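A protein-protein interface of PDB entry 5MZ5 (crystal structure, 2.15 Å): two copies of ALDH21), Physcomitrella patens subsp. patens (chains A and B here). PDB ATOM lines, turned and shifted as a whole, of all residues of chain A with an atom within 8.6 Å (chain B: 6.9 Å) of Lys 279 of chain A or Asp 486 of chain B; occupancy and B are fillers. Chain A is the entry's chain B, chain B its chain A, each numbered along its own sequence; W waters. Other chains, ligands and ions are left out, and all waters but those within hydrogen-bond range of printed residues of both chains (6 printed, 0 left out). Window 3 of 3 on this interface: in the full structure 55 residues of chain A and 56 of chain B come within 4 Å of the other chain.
Of the 19 printed residues of chain B, 5 touch a printed residue of chain A. Hydrophobic or aromatic side chains of chain B that line the printed part of chain A: Trp 271, Leu 484 and Ile 489. Among the printed residues, 7 pairs touch across the chains.
Water W1 bridges O of Trp 271 of chain B (2.7 Å) and O of Gly 278 of chain A (3.2 Å). Water W2 lies within hydrogen-bond range of the backbone carbonyl oxygen of Gly 278 of chain A and the side-chain amino group of Lys 274 of chain B. Water W4 bridges the side-chain amino group of Lys 274 of chain B (2.8 Å) and the backbone carbonyl oxygen of Lys 274 of chain A (2.9 Å). Water W5 bridges OD2 of Asp 486 of chain B and NZ of Lys 279 of chain A. Water W3 lies within hydrogen-bond range of the backbone NH of Lys 485 of chain B (2.8 Å) and the side-chain amino group of Lys 259 of chain A (2.9 Å). Water W6 bridges O of Gly 483 of chain B and OE2 of Glu 503 of chain A.
The indole nitrogen of Trp 271 of chain B sits at hydrogen-bond distance from the backbone carbonyl oxygen of Asp 486 of chain B (3.4 Å). OD2 of Asp 486 of chain B sits at hydrogen-bond distance from ND1 of His 439 of chain B (2.8 Å). The backbone carbonyl oxygen (O) of Thr 253 of chain A lies within hydrogen-bond range of the side-chain amino group (NZ) of Lys 280 of chain A (2.8 Å). The side-chain amino group of Lys 280 of chain A is in hydrogen-bond range of the backbone carbonyl oxygen of Asp 255 of chain A (2.8 Å). O of Ala 277 of chain A sits at hydrogen-bond distance from NZ of Lys 280 of chain A (2.8 Å). The side-chain amino group (NZ) of Lys 281 of chain A is in salt-bridge range of the side-chain carboxylate (OE2) of Glu 503 of chain A (3.7 Å).
Position printed for both chains: 274.
Lys 279 of chain A touches just these residues of chain B: Trp 271 (3.5 Å), Lys 274 (3.5 Å), Asp 486 (3.0 Å) and Ile 489 (3.9 Å). Asp 486 of chain B touches one residue of chain A. No residue of chain A comes within 4 Å of Ser 487 of chain B. Of the printed residues of chain B, Glu 503 of chain A touches Leu 484 (3.6 Å). Of the printed residues of chain A, Trp 271 of chain B touches Lys 279. Printed residues of chain B within 4 Å of Lys 280 of chain A: Lys 274. Printed residues of chain A within 4 Å of Leu 484 of chain B: Glu 503. Lys 485 of chain B touches none of the printed residues of chain A. The nearest residue of chain B that does not touch Lys 279 of chain A is Lys 485 of chain B (5.2 Å). The nearest printed residue of chain B that does not touch Lys 280 of chain A is Ile 489 of chain B (5.3 Å).
Lys 279 of chain A touches Trp 271 of chain B (O to CZ3, 3.5 Å). Lys 274 of chain B touches Lys 279 of chain A. Lys 279 of chain A touches Ile 489 of chain B. Glu 503 of chain A touches Leu 484 of chain B (CD to CD2, 3.6 Å).
O of Gly 278 of chain A is in hydrogen-bond range of NZ of Lys 274 of chain B. The side-chain amino group (NZ) of Lys 274 of chain B lies within hydrogen-bond range of the backbone carbonyl oxygen (O) of Lys 280 of chain A. NZ of Lys 279 of chain A lies within salt-bridge range of OD1 of Asp 486 of chain B (3.0 Å).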
ATOM      1  N   ILE A 179      19.292  -6.591 -15.194  1.00  0.00           N
ATOM      2  CA  ILE A 179      18.056  -5.807 -15.056  1.00  0.00           C
ATOM      3  C   ILE A 179      17.399  -5.532 -16.438  1.00  0.00           C
ATOM      4  O   ILE A 179      16.176  -5.449 -16.540  1.00  0.00           O
ATOM      5  CB  ILE A 179      18.286  -4.498 -14.221  1.00  0.00           C
ATOM      6  CG1 ILE A 179      16.930  -3.896 -13.712  1.00  0.00           C
ATOM      7  CG2 ILE A 179      19.159  -3.438 -14.979  1.00  0.00           C
ATOM      8  CD1 ILE A 179      17.097  -2.783 -12.641  1.00  0.00           C
ATOM      9  N   THR A 253      15.015   9.735 -19.727  1.00  0.00           N
ATOM     10  CA  THR A 253      14.364   9.744 -18.419  1.00  0.00           C
ATOM     11  C   THR A 253      13.078   8.932 -18.396  1.00  0.00           C
ATOM     12  O   THR A 253      12.916   8.074 -17.531  1.00  0.00           O
ATOM     13  CB  THR A 253      14.116  11.212 -17.973  1.00  0.00           C
ATOM     14  OG1 THR A 253      15.373  11.834 -17.779  1.00  0.00           O
ATOM     15  CG2 THR A 253      13.313  11.324 -16.695  1.00  0.00           C
ATOM     16  N   VAL A 254      12.151   9.242 -19.311  1.00  0.00           N
ATOM     17  CA  VAL A 254      10.784   8.711 -19.308  1.00  0.00           C
ATOM     18  C   VAL A 254      10.573   7.376 -20.022  1.00  0.00           C
ATOM     19  O   VAL A 254       9.596   6.701 -19.689  1.00  0.00           O
ATOM     20  CB  VAL A 254       9.766   9.763 -19.848  1.00  0.00           C
ATOM     21  CG1 VAL A 254       9.861  11.065 -19.070  1.00  0.00           C
ATOM     22  CG2 VAL A 254       9.949  10.017 -21.349  1.00  0.00           C
ATOM     23  N   ASP A 255      11.424   7.003 -20.992  1.00  0.00           N
ATOM     24  CA  ASP A 255      11.154   5.806 -21.787  1.00  0.00           C
ATOM     25  C   ASP A 255      11.014   4.526 -20.949  1.00  0.00           C
ATOM     26  O   ASP A 255      11.914   4.160 -20.196  1.00  0.00           O
ATOM     27  CB  ASP A 255      12.137   5.622 -22.945  1.00  0.00           C
ATOM     28  CG  ASP A 255      11.501   4.818 -24.054  1.00  0.00           C
ATOM     29  OD1 ASP A 255      11.468   3.584 -23.938  1.00  0.00           O
ATOM     30  OD2 ASP A 255      10.966   5.433 -25.001  1.00  0.00           O
ATOM     31  N   GLU A 256       9.832   3.882 -21.070  1.00  0.00           N
ATOM     32  CA  GLU A 256       9.471   2.688 -20.323  1.00  0.00           C
ATOM     33  C   GLU A 256      10.271   1.439 -20.714  1.00  0.00           C
ATOM     34  O   GLU A 256      10.307   0.497 -19.929  1.00  0.00           O
ATOM     35  CB  GLU A 256       7.964   2.437 -20.417  1.00  0.00           C
ATOM     36  CG  GLU A 256       7.375   1.921 -19.112  1.00  0.00           C
ATOM     37  CD  GLU A 256       5.860   1.847 -18.981  1.00  0.00           C
ATOM     38  OE1 GLU A 256       5.401   1.263 -17.974  1.00  0.00           O
ATOM     39  OE2 GLU A 256       5.134   2.371 -19.860  1.00  0.00           O
ATOM     40  N   PHE A 258      13.474   1.281 -20.911  1.00  0.00           N
ATOM     41  CA  PHE A 258      14.646   1.290 -20.052  1.00  0.00           C
ATOM     42  C   PHE A 258      14.255   0.742 -18.670  1.00  0.00           C
ATOM     43  O   PHE A 258      13.219   1.116 -18.125  1.00  0.00           O
ATOM     44  CB  PHE A 258      15.246   2.705 -19.905  1.00  0.00           C
ATOM     45  CG  PHE A 258      15.962   3.328 -21.088  1.00  0.00           C
ATOM     46  CD1 PHE A 258      17.086   2.713 -21.650  1.00  0.00           C
ATOM     47  CD2 PHE A 258      15.572   4.578 -21.579  1.00  0.00           C
ATOM     48  CE1 PHE A 258      17.782   3.325 -22.704  1.00  0.00           C
ATOM     49  CE2 PHE A 258      16.283   5.198 -22.619  1.00  0.00           C
ATOM     50  CZ  PHE A 258      17.383   4.575 -23.170  1.00  0.00           C
ATOM     51  N   LYS A 259      15.092  -0.115 -18.100  1.00  0.00           N
ATOM     52  CA  LYS A 259      14.823  -0.709 -16.782  1.00  0.00           C
ATOM     53  C   LYS A 259      15.556   0.033 -15.676  1.00  0.00           C
ATOM     54  O   LYS A 259      15.206  -0.085 -14.502  1.00  0.00           O
ATOM     55  CB  LYS A 259      15.196  -2.204 -16.786  1.00  0.00           C
ATOM     56  CG  LYS A 259      14.372  -3.041 -17.792  1.00  0.00           C
ATOM     57  CD  LYS A 259      12.847  -2.972 -17.587  1.00  0.00           C
ATOM     58  CE  LYS A 259      12.311  -3.869 -16.508  1.00  0.00           C
ATOM     59  NZ  LYS A 259      10.818  -3.855 -16.462  1.00  0.00           N
ATOM     60  N   LEU A 260      16.590   0.777 -16.055  1.00  0.00           N
ATOM     61  CA  LEU A 260      17.392   1.553 -15.135  1.00  0.00           C
ATOM     62  C   LEU A 260      17.873   2.841 -15.784  1.00  0.00           C
ATOM     63  O   LEU A 260      18.294   2.846 -16.940  1.00  0.00           O
ATOM     64  CB  LEU A 260      18.603   0.710 -14.653  1.00  0.00           C
ATOM     65  CG  LEU A 260      19.691   1.422 -13.797  1.00  0.00           C
ATOM     66  CD1 LEU A 260      19.208   1.738 -12.385  1.00  0.00           C
ATOM     67  CD2 LEU A 260      20.916   0.552 -13.674  1.00  0.00           C
ATOM     68  N   LEU A 261      17.823   3.920 -15.020  1.00  0.00           N
ATOM     69  CA  LEU A 261      18.390   5.204 -15.394  1.00  0.00           C
ATOM     70  C   LEU A 261      19.570   5.442 -14.456  1.00  0.00           C
ATOM     71  O   LEU A 261      19.395   5.429 -13.230  1.00  0.00           O
ATOM     72  CB  LEU A 261      17.366   6.364 -15.256  1.00  0.00           C
ATOM     73  CG  LEU A 261      17.944   7.805 -15.205  1.00  0.00           C
ATOM     74  CD1 LEU A 261      18.664   8.178 -16.520  1.00  0.00           C
ATOM     75  CD2 LEU A 261      16.854   8.827 -14.853  1.00  0.00           C
ATOM     76  N   LYS A 274      14.673  11.960 -11.606  1.00  0.00           N
ATOM     77  CA  LYS A 274      14.155  10.936 -10.694  1.00  0.00           C
ATOM     78  C   LYS A 274      12.624  11.081 -10.574  1.00  0.00           C
ATOM     79  O   LYS A 274      11.906  10.073 -10.641  1.00  0.00           O
ATOM     80  CB  LYS A 274      14.820  11.044  -9.305  1.00  0.00           C
ATOM     81  CG  LYS A 274      14.390   9.941  -8.324  1.00  0.00           C
ATOM     82  CD  LYS A 274      14.952  10.185  -6.931  1.00  0.00           C
ATOM     83  CE  LYS A 274      14.614   9.098  -5.934  1.00  0.00           C
ATOM     84  NZ  LYS A 274      13.240   9.255  -5.384  1.00  0.00           N
ATOM     85  N   ALA A 275      12.138  12.330 -10.466  1.00  0.00           N
ATOM     86  CA  ALA A 275      10.700  12.650 -10.357  1.00  0.00           C
ATOM     87  C   ALA A 275       9.903  12.238 -11.601  1.00  0.00           C
ATOM     88  O   ALA A 275       8.746  11.822 -11.484  1.00  0.00           O
ATOM     89  CB  ALA A 275      10.510  14.140 -10.073  1.00  0.00           C
ATOM     90  N   ARG A 276      10.553  12.274 -12.777  1.00  0.00           N
ATOM     91  CA  ARG A 276       9.917  11.975 -14.064  1.00  0.00           C
ATOM     92  C   ARG A 276      10.281  10.619 -14.667  1.00  0.00           C
ATOM     93  O   ARG A 276       9.841  10.319 -15.777  1.00  0.00           O
ATOM     94  CB  ARG A 276      10.251  13.101 -15.068  1.00  0.00           C
ATOM     95  CG  ARG A 276       9.715  14.469 -14.668  1.00  0.00           C
ATOM     96  CD  ARG A 276       9.969  15.526 -15.738  1.00  0.00           C
ATOM     97  NE  ARG A 276      11.387  15.886 -15.762  1.00  0.00           N
ATOM     98  CZ  ARG A 276      12.255  15.506 -16.693  1.00  0.00           C
ATOM     99  NH1 ARG A 276      11.847  14.804 -17.747  1.00  0.00           N
ATOM    100  NH2 ARG A 276      13.538  15.834 -16.585  1.00  0.00           N
ATOM    101  N   ALA A 277      11.101   9.810 -13.964  1.00  0.00           N
ATOM    102  CA  ALA A 277      11.606   8.552 -14.507  1.00  0.00           C
ATOM    103  C   ALA A 277      10.565   7.463 -14.753  1.00  0.00           C
ATOM    104  O   ALA A 277      10.801   6.597 -15.601  1.00  0.00           O
ATOM    105  CB  ALA A 277      12.735   8.005 -13.646  1.00  0.00           C
ATOM    106  N   GLY A 278       9.428   7.508 -14.064  1.00  0.00           N
ATOM    107  CA  GLY A 278       8.430   6.456 -14.248  1.00  0.00           C
ATOM    108  C   GLY A 278       8.761   5.250 -13.387  1.00  0.00           C
ATOM    109  O   GLY A 278       9.301   5.416 -12.297  1.00  0.00           O
ATOM    110  N   LYS A 279       8.524   4.033 -13.895  1.00  0.00           N
ATOM    111  CA  LYS A 279       8.695   2.767 -13.148  1.00  0.00           C
ATOM    112  C   LYS A 279      10.130   2.313 -12.908  1.00  0.00           C
ATOM    113  O   LYS A 279      10.384   1.667 -11.892  1.00  0.00           O
ATOM    114  CB  LYS A 279       7.895   1.618 -13.803  1.00  0.00           C
ATOM    115  CG  LYS A 279       6.404   1.908 -13.817  1.00  0.00           C
ATOM    116  CD  LYS A 279       5.605   0.843 -14.518  1.00  0.00           C
ATOM    117  CE  LYS A 279       4.139   1.193 -14.510  1.00  0.00           C
ATOM    118  NZ  LYS A 279       3.440   0.590 -15.667  1.00  0.00           N
ATOM    119  N   LYS A 280      11.054   2.661 -13.811  1.00  0.00           N
ATOM    120  CA  LYS A 280      12.466   2.251 -13.755  1.00  0.00           C
ATOM    121  C   LYS A 280      13.201   2.608 -12.460  1.00  0.00           C
ATOM    122  O   LYS A 280      12.870   3.598 -11.789  1.00  0.00           O
ATOM    123  CB  LYS A 280      13.245   2.812 -14.968  1.00  0.00           C
ATOM    124  CG  LYS A 280      13.318   4.350 -14.994  1.00  0.00           C
ATOM    125  CD  LYS A 280      14.183   4.931 -16.097  1.00  0.00           C
ATOM    126  CE  LYS A 280      13.638   4.816 -17.495  1.00  0.00           C
ATOM    127  NZ  LYS A 280      12.254   5.348 -17.649  1.00  0.00           N
ATOM    128  N   LYS A 281      14.235   1.816 -12.149  1.00  0.00           N
ATOM    129  CA  LYS A 281      15.146   2.085 -11.047  1.00  0.00           C
ATOM    130  C   LYS A 281      16.026   3.285 -11.448  1.00  0.00           C
ATOM    131  O   LYS A 281      16.276   3.512 -12.635  1.00  0.00           O
ATOM    132  CB  LYS A 281      15.997   0.861 -10.695  1.00  0.00           C
ATOM    133  CG  LYS A 281      15.216  -0.180  -9.911  1.00  0.00           C
ATOM    134  CD  LYS A 281      16.126  -1.241  -9.328  1.00  0.00           C
ATOM    135  CE  LYS A 281      15.359  -2.486  -8.937  1.00  0.00           C
ATOM    136  NZ  LYS A 281      16.136  -3.342  -7.998  1.00  0.00           N
ATOM    137  N   VAL A 282      16.405   4.098 -10.469  1.00  0.00           N
ATOM    138  CA  VAL A 282      17.179   5.318 -10.692  1.00  0.00           C
ATOM    139  C   VAL A 282      18.448   5.308  -9.828  1.00  0.00           C
ATOM    140  O   VAL A 282      18.343   5.083  -8.640  1.00  0.00           O
ATOM    141  CB  VAL A 282      16.270   6.574 -10.453  1.00  0.00           C
ATOM    142  CG1 VAL A 282      17.065   7.867 -10.454  1.00  0.00           C
ATOM    143  CG2 VAL A 282      15.164   6.656 -11.499  1.00  0.00           C
ATOM    144  N   GLU A 503      19.086  -8.056 -10.955  1.00  0.00           N
ATOM    145  CA  GLU A 503      17.833  -8.369 -10.275  1.00  0.00           C
ATOM    146  C   GLU A 503      17.960  -9.720  -9.603  1.00  0.00           C
ATOM    147  O   GLU A 503      18.513 -10.657 -10.174  1.00  0.00           O
ATOM    148  CB  GLU A 503      16.627  -8.335 -11.229  1.00  0.00           C
ATOM    149  CG  GLU A 503      16.075  -6.935 -11.412  1.00  0.00           C
ATOM    150  CD  GLU A 503      15.211  -6.368 -10.293  1.00  0.00           C
ATOM    151  OE1 GLU A 503      15.186  -6.928  -9.170  1.00  0.00           O
ATOM    152  OE2 GLU A 503      14.490  -5.386 -10.576  1.00  0.00           O
ATOM    153  N   GLY B 267      -0.971  -1.436  -7.393  1.00  0.00           N
ATOM    154  CA  GLY B 267      -0.005  -1.005  -8.396  1.00  0.00           C
ATOM    155  C   GLY B 267      -0.174   0.429  -8.856  1.00  0.00           C
ATOM    156  O   GLY B 267       0.774   1.204  -8.722  1.00  0.00           O
ATOM    157  N   PRO B 268      -1.378   0.846  -9.363  1.00  0.00           N
ATOM    158  CA  PRO B 268      -1.535   2.239  -9.821  1.00  0.00           C
ATOM    159  C   PRO B 268      -1.264   3.275  -8.736  1.00  0.00           C
ATOM    160  O   PRO B 268      -0.684   4.321  -9.015  1.00  0.00           O
ATOM    161  CB  PRO B 268      -2.988   2.294 -10.327  1.00  0.00           C
ATOM    162  CG  PRO B 268      -3.335   0.894 -10.631  1.00  0.00           C
ATOM    163  CD  PRO B 268      -2.603   0.058  -9.621  1.00  0.00           C
ATOM    164  N   TRP B 271       2.829   3.055  -8.009  1.00  0.00           N
ATOM    165  CA  TRP B 271       3.607   3.736  -9.049  1.00  0.00           C
ATOM    166  C   TRP B 271       3.462   5.251  -8.999  1.00  0.00           C
ATOM    167  O   TRP B 271       4.437   5.956  -9.202  1.00  0.00           O
ATOM    168  CB  TRP B 271       3.295   3.177 -10.455  1.00  0.00           C
ATOM    169  CG  TRP B 271       3.747   1.752 -10.625  1.00  0.00           C
ATOM    170  CD1 TRP B 271       2.966   0.673 -10.928  1.00  0.00           C
ATOM    171  CD2 TRP B 271       5.084   1.246 -10.465  1.00  0.00           C
ATOM    172  NE1 TRP B 271       3.735  -0.456 -11.025  1.00  0.00           N
ATOM    173  CE2 TRP B 271       5.042  -0.137 -10.751  1.00  0.00           C
ATOM    174  CE3 TRP B 271       6.321   1.836 -10.141  1.00  0.00           C
ATOM    175  CZ2 TRP B 271       6.191  -0.939 -10.733  1.00  0.00           C
ATOM    176  CZ3 TRP B 271       7.457   1.038 -10.114  1.00  0.00           C
ATOM    177  CH2 TRP B 271       7.386  -0.331 -10.393  1.00  0.00           C
ATOM    178  N   LYS B 274       5.559   6.529  -6.058  1.00  0.00           N
ATOM    179  CA  LYS B 274       6.982   6.521  -6.455  1.00  0.00           C
ATOM    180  C   LYS B 274       7.297   7.783  -7.278  1.00  0.00           C
ATOM    181  O   LYS B 274       8.288   8.456  -6.989  1.00  0.00           O
ATOM    182  CB  LYS B 274       7.318   5.236  -7.253  1.00  0.00           C
ATOM    183  CG  LYS B 274       8.794   5.113  -7.642  1.00  0.00           C
ATOM    184  CD  LYS B 274       9.016   3.975  -8.637  1.00  0.00           C
ATOM    185  CE  LYS B 274      10.463   3.821  -9.089  1.00  0.00           C
ATOM    186  NZ  LYS B 274      10.867   4.836 -10.102  1.00  0.00           N
ATOM    187  N   GLU B 285       5.946  -3.147  -3.098  1.00  0.00           N
ATOM    188  CA  GLU B 285       5.474  -4.531  -3.183  1.00  0.00           C
ATOM    189  C   GLU B 285       4.063  -4.420  -3.720  1.00  0.00           C
ATOM    190  O   GLU B 285       3.159  -3.964  -3.014  1.00  0.00           O
ATOM    191  CB  GLU B 285       5.504  -5.230  -1.817  1.00  0.00           C
ATOM    192  CG  GLU B 285       6.903  -5.480  -1.291  1.00  0.00           C
ATOM    193  CD  GLU B 285       7.731  -6.514  -2.040  1.00  0.00           C
ATOM    194  OE1 GLU B 285       8.976  -6.450  -1.943  1.00  0.00           O
ATOM    195  OE2 GLU B 285       7.141  -7.375  -2.734  1.00  0.00           O
ATOM    196  N   LEU B 286       3.898  -4.705  -5.016  1.00  0.00           N
ATOM    197  CA  LEU B 286       2.594  -4.526  -5.668  1.00  0.00           C
ATOM    198  C   LEU B 286       2.016  -5.865  -6.089  1.00  0.00           C
ATOM    199  O   LEU B 286       2.527  -6.901  -5.653  1.00  0.00           O
ATOM    200  CB  LEU B 286       2.677  -3.485  -6.814  1.00  0.00           C
ATOM    201  CG  LEU B 286       3.528  -2.230  -6.493  1.00  0.00           C
ATOM    202  CD1 LEU B 286       3.805  -1.433  -7.715  1.00  0.00           C
ATOM    203  CD2 LEU B 286       2.906  -1.365  -5.372  1.00  0.00           C
ATOM    204  N   GLY B 287       0.956  -5.843  -6.880  1.00  0.00           N
ATOM    205  CA  GLY B 287       0.255  -7.057  -7.288  1.00  0.00           C
ATOM    206  C   GLY B 287       0.952  -8.001  -8.247  1.00  0.00           C
ATOM    207  O   GLY B 287       2.111  -7.801  -8.621  1.00  0.00           O
ATOM    208  N   GLY B 288       0.230  -9.042  -8.640  1.00  0.00           N
ATOM    209  CA  GLY B 288       0.724 -10.022  -9.585  1.00  0.00           C
ATOM    210  C   GLY B 288      -0.366 -10.712 -10.364  1.00  0.00           C
ATOM    211  O   GLY B 288      -1.551 -10.467 -10.149  1.00  0.00           O
ATOM    212  N   GLU B 413      -5.474  -8.518 -16.194  1.00  0.00           N
ATOM    213  CA  GLU B 413      -5.277  -7.884 -14.890  1.00  0.00           C
ATOM    214  C   GLU B 413      -5.301  -8.859 -13.724  1.00  0.00           C
ATOM    215  O   GLU B 413      -5.766  -9.991 -13.859  1.00  0.00           O
ATOM    216  CB  GLU B 413      -6.369  -6.807 -14.647  1.00  0.00           C
ATOM    217  CG  GLU B 413      -6.638  -5.846 -15.793  1.00  0.00           C
ATOM    218  CD  GLU B 413      -5.497  -4.936 -16.202  1.00  0.00           C
ATOM    219  OE1 GLU B 413      -4.612  -4.650 -15.363  1.00  0.00           O
ATOM    220  OE2 GLU B 413      -5.501  -4.491 -17.371  1.00  0.00           O
ATOM    221  N   HIS B 439       2.010  -8.189 -17.717  1.00  0.00           N
ATOM    222  CA  HIS B 439       2.671  -6.949 -17.321  1.00  0.00           C
ATOM    223  C   HIS B 439       3.098  -6.998 -15.848  1.00  0.00           C
ATOM    224  O   HIS B 439       3.744  -6.077 -15.350  1.00  0.00           O
ATOM    225  CB  HIS B 439       1.843  -5.702 -17.683  1.00  0.00           C
ATOM    226  CG  HIS B 439       0.469  -5.627 -17.075  1.00  0.00           C
ATOM    227  ND1 HIS B 439       0.225  -4.892 -15.908  1.00  0.00           N
ATOM    228  CD2 HIS B 439      -0.712  -6.092 -17.548  1.00  0.00           C
ATOM    229  CE1 HIS B 439      -1.086  -4.950 -15.709  1.00  0.00           C
ATOM    230  NE2 HIS B 439      -1.693  -5.672 -16.660  1.00  0.00           N
ATOM    231  N   TYR B 440       2.816  -8.126 -15.178  1.00  0.00           N
ATOM    232  CA  TYR B 440       3.241  -8.395 -13.798  1.00  0.00           C
ATOM    233  C   TYR B 440       4.467  -9.328 -13.843  1.00  0.00           C
ATOM    234  O   TYR B 440       4.821  -9.821 -14.915  1.00  0.00           O
ATOM    235  CB  TYR B 440       2.095  -9.031 -13.004  1.00  0.00           C
ATOM    236  CG  TYR B 440       0.821  -8.209 -12.958  1.00  0.00           C
ATOM    237  CD1 TYR B 440       0.641  -7.213 -11.999  1.00  0.00           C
ATOM    238  CD2 TYR B 440      -0.213  -8.441 -13.860  1.00  0.00           C
ATOM    239  CE1 TYR B 440      -0.546  -6.473 -11.938  1.00  0.00           C
ATOM    240  CE2 TYR B 440      -1.408  -7.724 -13.797  1.00  0.00           C
ATOM    241  CZ  TYR B 440      -1.570  -6.736 -12.836  1.00  0.00           C
ATOM    242  OH  TYR B 440      -2.747  -6.015 -12.797  1.00  0.00           O
ATOM    243  N   GLY B 441       5.117  -9.547 -12.700  1.00  0.00           N
ATOM    244  CA  GLY B 441       6.286 -10.419 -12.624  1.00  0.00           C
ATOM    245  C   GLY B 441       6.718 -10.719 -11.211  1.00  0.00           C
ATOM    246  O   GLY B 441       7.885 -10.550 -10.871  1.00  0.00           O
ATOM    247  N   GLY B 483       9.120  -8.430  -7.095  1.00  0.00           N
ATOM    248  CA  GLY B 483       9.045  -8.746  -8.509  1.00  0.00           C
ATOM    249  C   GLY B 483       9.604  -7.786  -9.523  1.00  0.00           C
ATOM    250  O   GLY B 483      10.245  -6.780  -9.206  1.00  0.00           O
ATOM    251  N   LEU B 484       9.353  -8.162 -10.770  1.00  0.00           N
ATOM    252  CA  LEU B 484       9.745  -7.431 -11.961  1.00  0.00           C
ATOM    253  C   LEU B 484       8.499  -6.815 -12.539  1.00  0.00           C
ATOM    254  O   LEU B 484       7.388  -7.073 -12.043  1.00  0.00           O
ATOM    255  CB  LEU B 484      10.400  -8.402 -12.986  1.00  0.00           C
ATOM    256  CG  LEU B 484      11.593  -9.245 -12.496  1.00  0.00           C
ATOM    257  CD1 LEU B 484      12.206 -10.039 -13.659  1.00  0.00           C
ATOM    258  CD2 LEU B 484      12.660  -8.385 -11.820  1.00  0.00           C
ATOM    259  N   LYS B 485       8.683  -5.982 -13.574  1.00  0.00           N
ATOM    260  CA  LYS B 485       7.617  -5.312 -14.311  1.00  0.00           C
ATOM    261  C   LYS B 485       6.680  -4.481 -13.377  1.00  0.00           C
ATOM    262  O   LYS B 485       7.187  -3.682 -12.584  1.00  0.00           O
ATOM    263  CB  LYS B 485       6.862  -6.325 -15.202  1.00  0.00           C
ATOM    264  CG  LYS B 485       7.752  -7.190 -16.113  1.00  0.00           C
ATOM    265  CD  LYS B 485       6.864  -8.086 -16.993  1.00  0.00           C
ATOM    266  CE  LYS B 485       7.618  -9.238 -17.575  1.00  0.00           C
ATOM    267  NZ  LYS B 485       6.707 -10.180 -18.284  1.00  0.00           N
ATOM    268  N   ASP B 486       5.344  -4.657 -13.462  1.00  0.00           N
ATOM    269  CA  ASP B 486       4.402  -3.879 -12.640  1.00  0.00           C
ATOM    270  C   ASP B 486       4.233  -4.391 -11.211  1.00  0.00           C
ATOM    271  O   ASP B 486       3.518  -3.760 -10.422  1.00  0.00           O
ATOM    272  CB  ASP B 486       3.031  -3.734 -13.329  1.00  0.00           C
ATOM    273  CG  ASP B 486       3.055  -2.888 -14.595  1.00  0.00           C
ATOM    274  OD1 ASP B 486       4.114  -2.265 -14.885  1.00  0.00           O
ATOM    275  OD2 ASP B 486       2.019  -2.835 -15.288  1.00  0.00           O
ATOM    276  N   SER B 487       4.932  -5.478 -10.858  1.00  0.00           N
ATOM    277  CA  SER B 487       4.864  -6.073  -9.516  1.00  0.00           C
ATOM    278  C   SER B 487       5.667  -5.305  -8.445  1.00  0.00           C
ATOM    279  O   SER B 487       5.491  -5.555  -7.262  1.00  0.00           O
ATOM    280  CB  SER B 487       5.232  -7.549  -9.557  1.00  0.00           C
ATOM    281  OG  SER B 487       4.204  -8.205 -10.279  1.00  0.00           O
ATOM    282  N   GLY B 488       6.464  -4.336  -8.862  1.00  0.00           N
ATOM    283  CA  GLY B 488       7.175  -3.449  -7.942  1.00  0.00           C
ATOM    284  C   GLY B 488       8.658  -3.300  -8.186  1.00  0.00           C
ATOM    285  O   GLY B 488       9.152  -3.600  -9.276  1.00  0.00           O
ATOM    286  N   ILE B 489       9.357  -2.806  -7.164  1.00  0.00           N
ATOM    287  CA  ILE B 489      10.813  -2.610  -7.128  1.00  0.00           C
ATOM    288  C   ILE B 489      11.357  -3.013  -5.762  1.00  0.00           C
ATOM    289  O   ILE B 489      10.741  -2.709  -4.727  1.00  0.00           O
ATOM    290  CB  ILE B 489      11.302  -1.195  -7.575  1.00  0.00           C
ATOM    291  CG1 ILE B 489      10.559  -0.056  -6.853  1.00  0.00           C
ATOM    292  CG2 ILE B 489      11.226  -1.009  -9.113  1.00  0.00           C
ATOM    293  CD1 ILE B 489      11.420   1.156  -6.689  1.00  0.00           C
HETATM  294  O   HOH W   1       6.377   5.407 -10.975  1.00  0.00           O
HETATM  295  O   HOH W   2       8.859   7.558 -10.587  1.00  0.00           O
HETATM  296  O   HOH W   3      11.074  -4.502 -13.689  1.00  0.00           O
HETATM  297  O   HOH W   4      11.763   7.399  -9.513  1.00  0.00           O
HETATM  298  O   HOH W   5       2.700  -1.974 -17.872  1.00  0.00           O
HETATM  299  O   HOH W   6      12.410  -5.056  -8.663  1.00  0.00           O
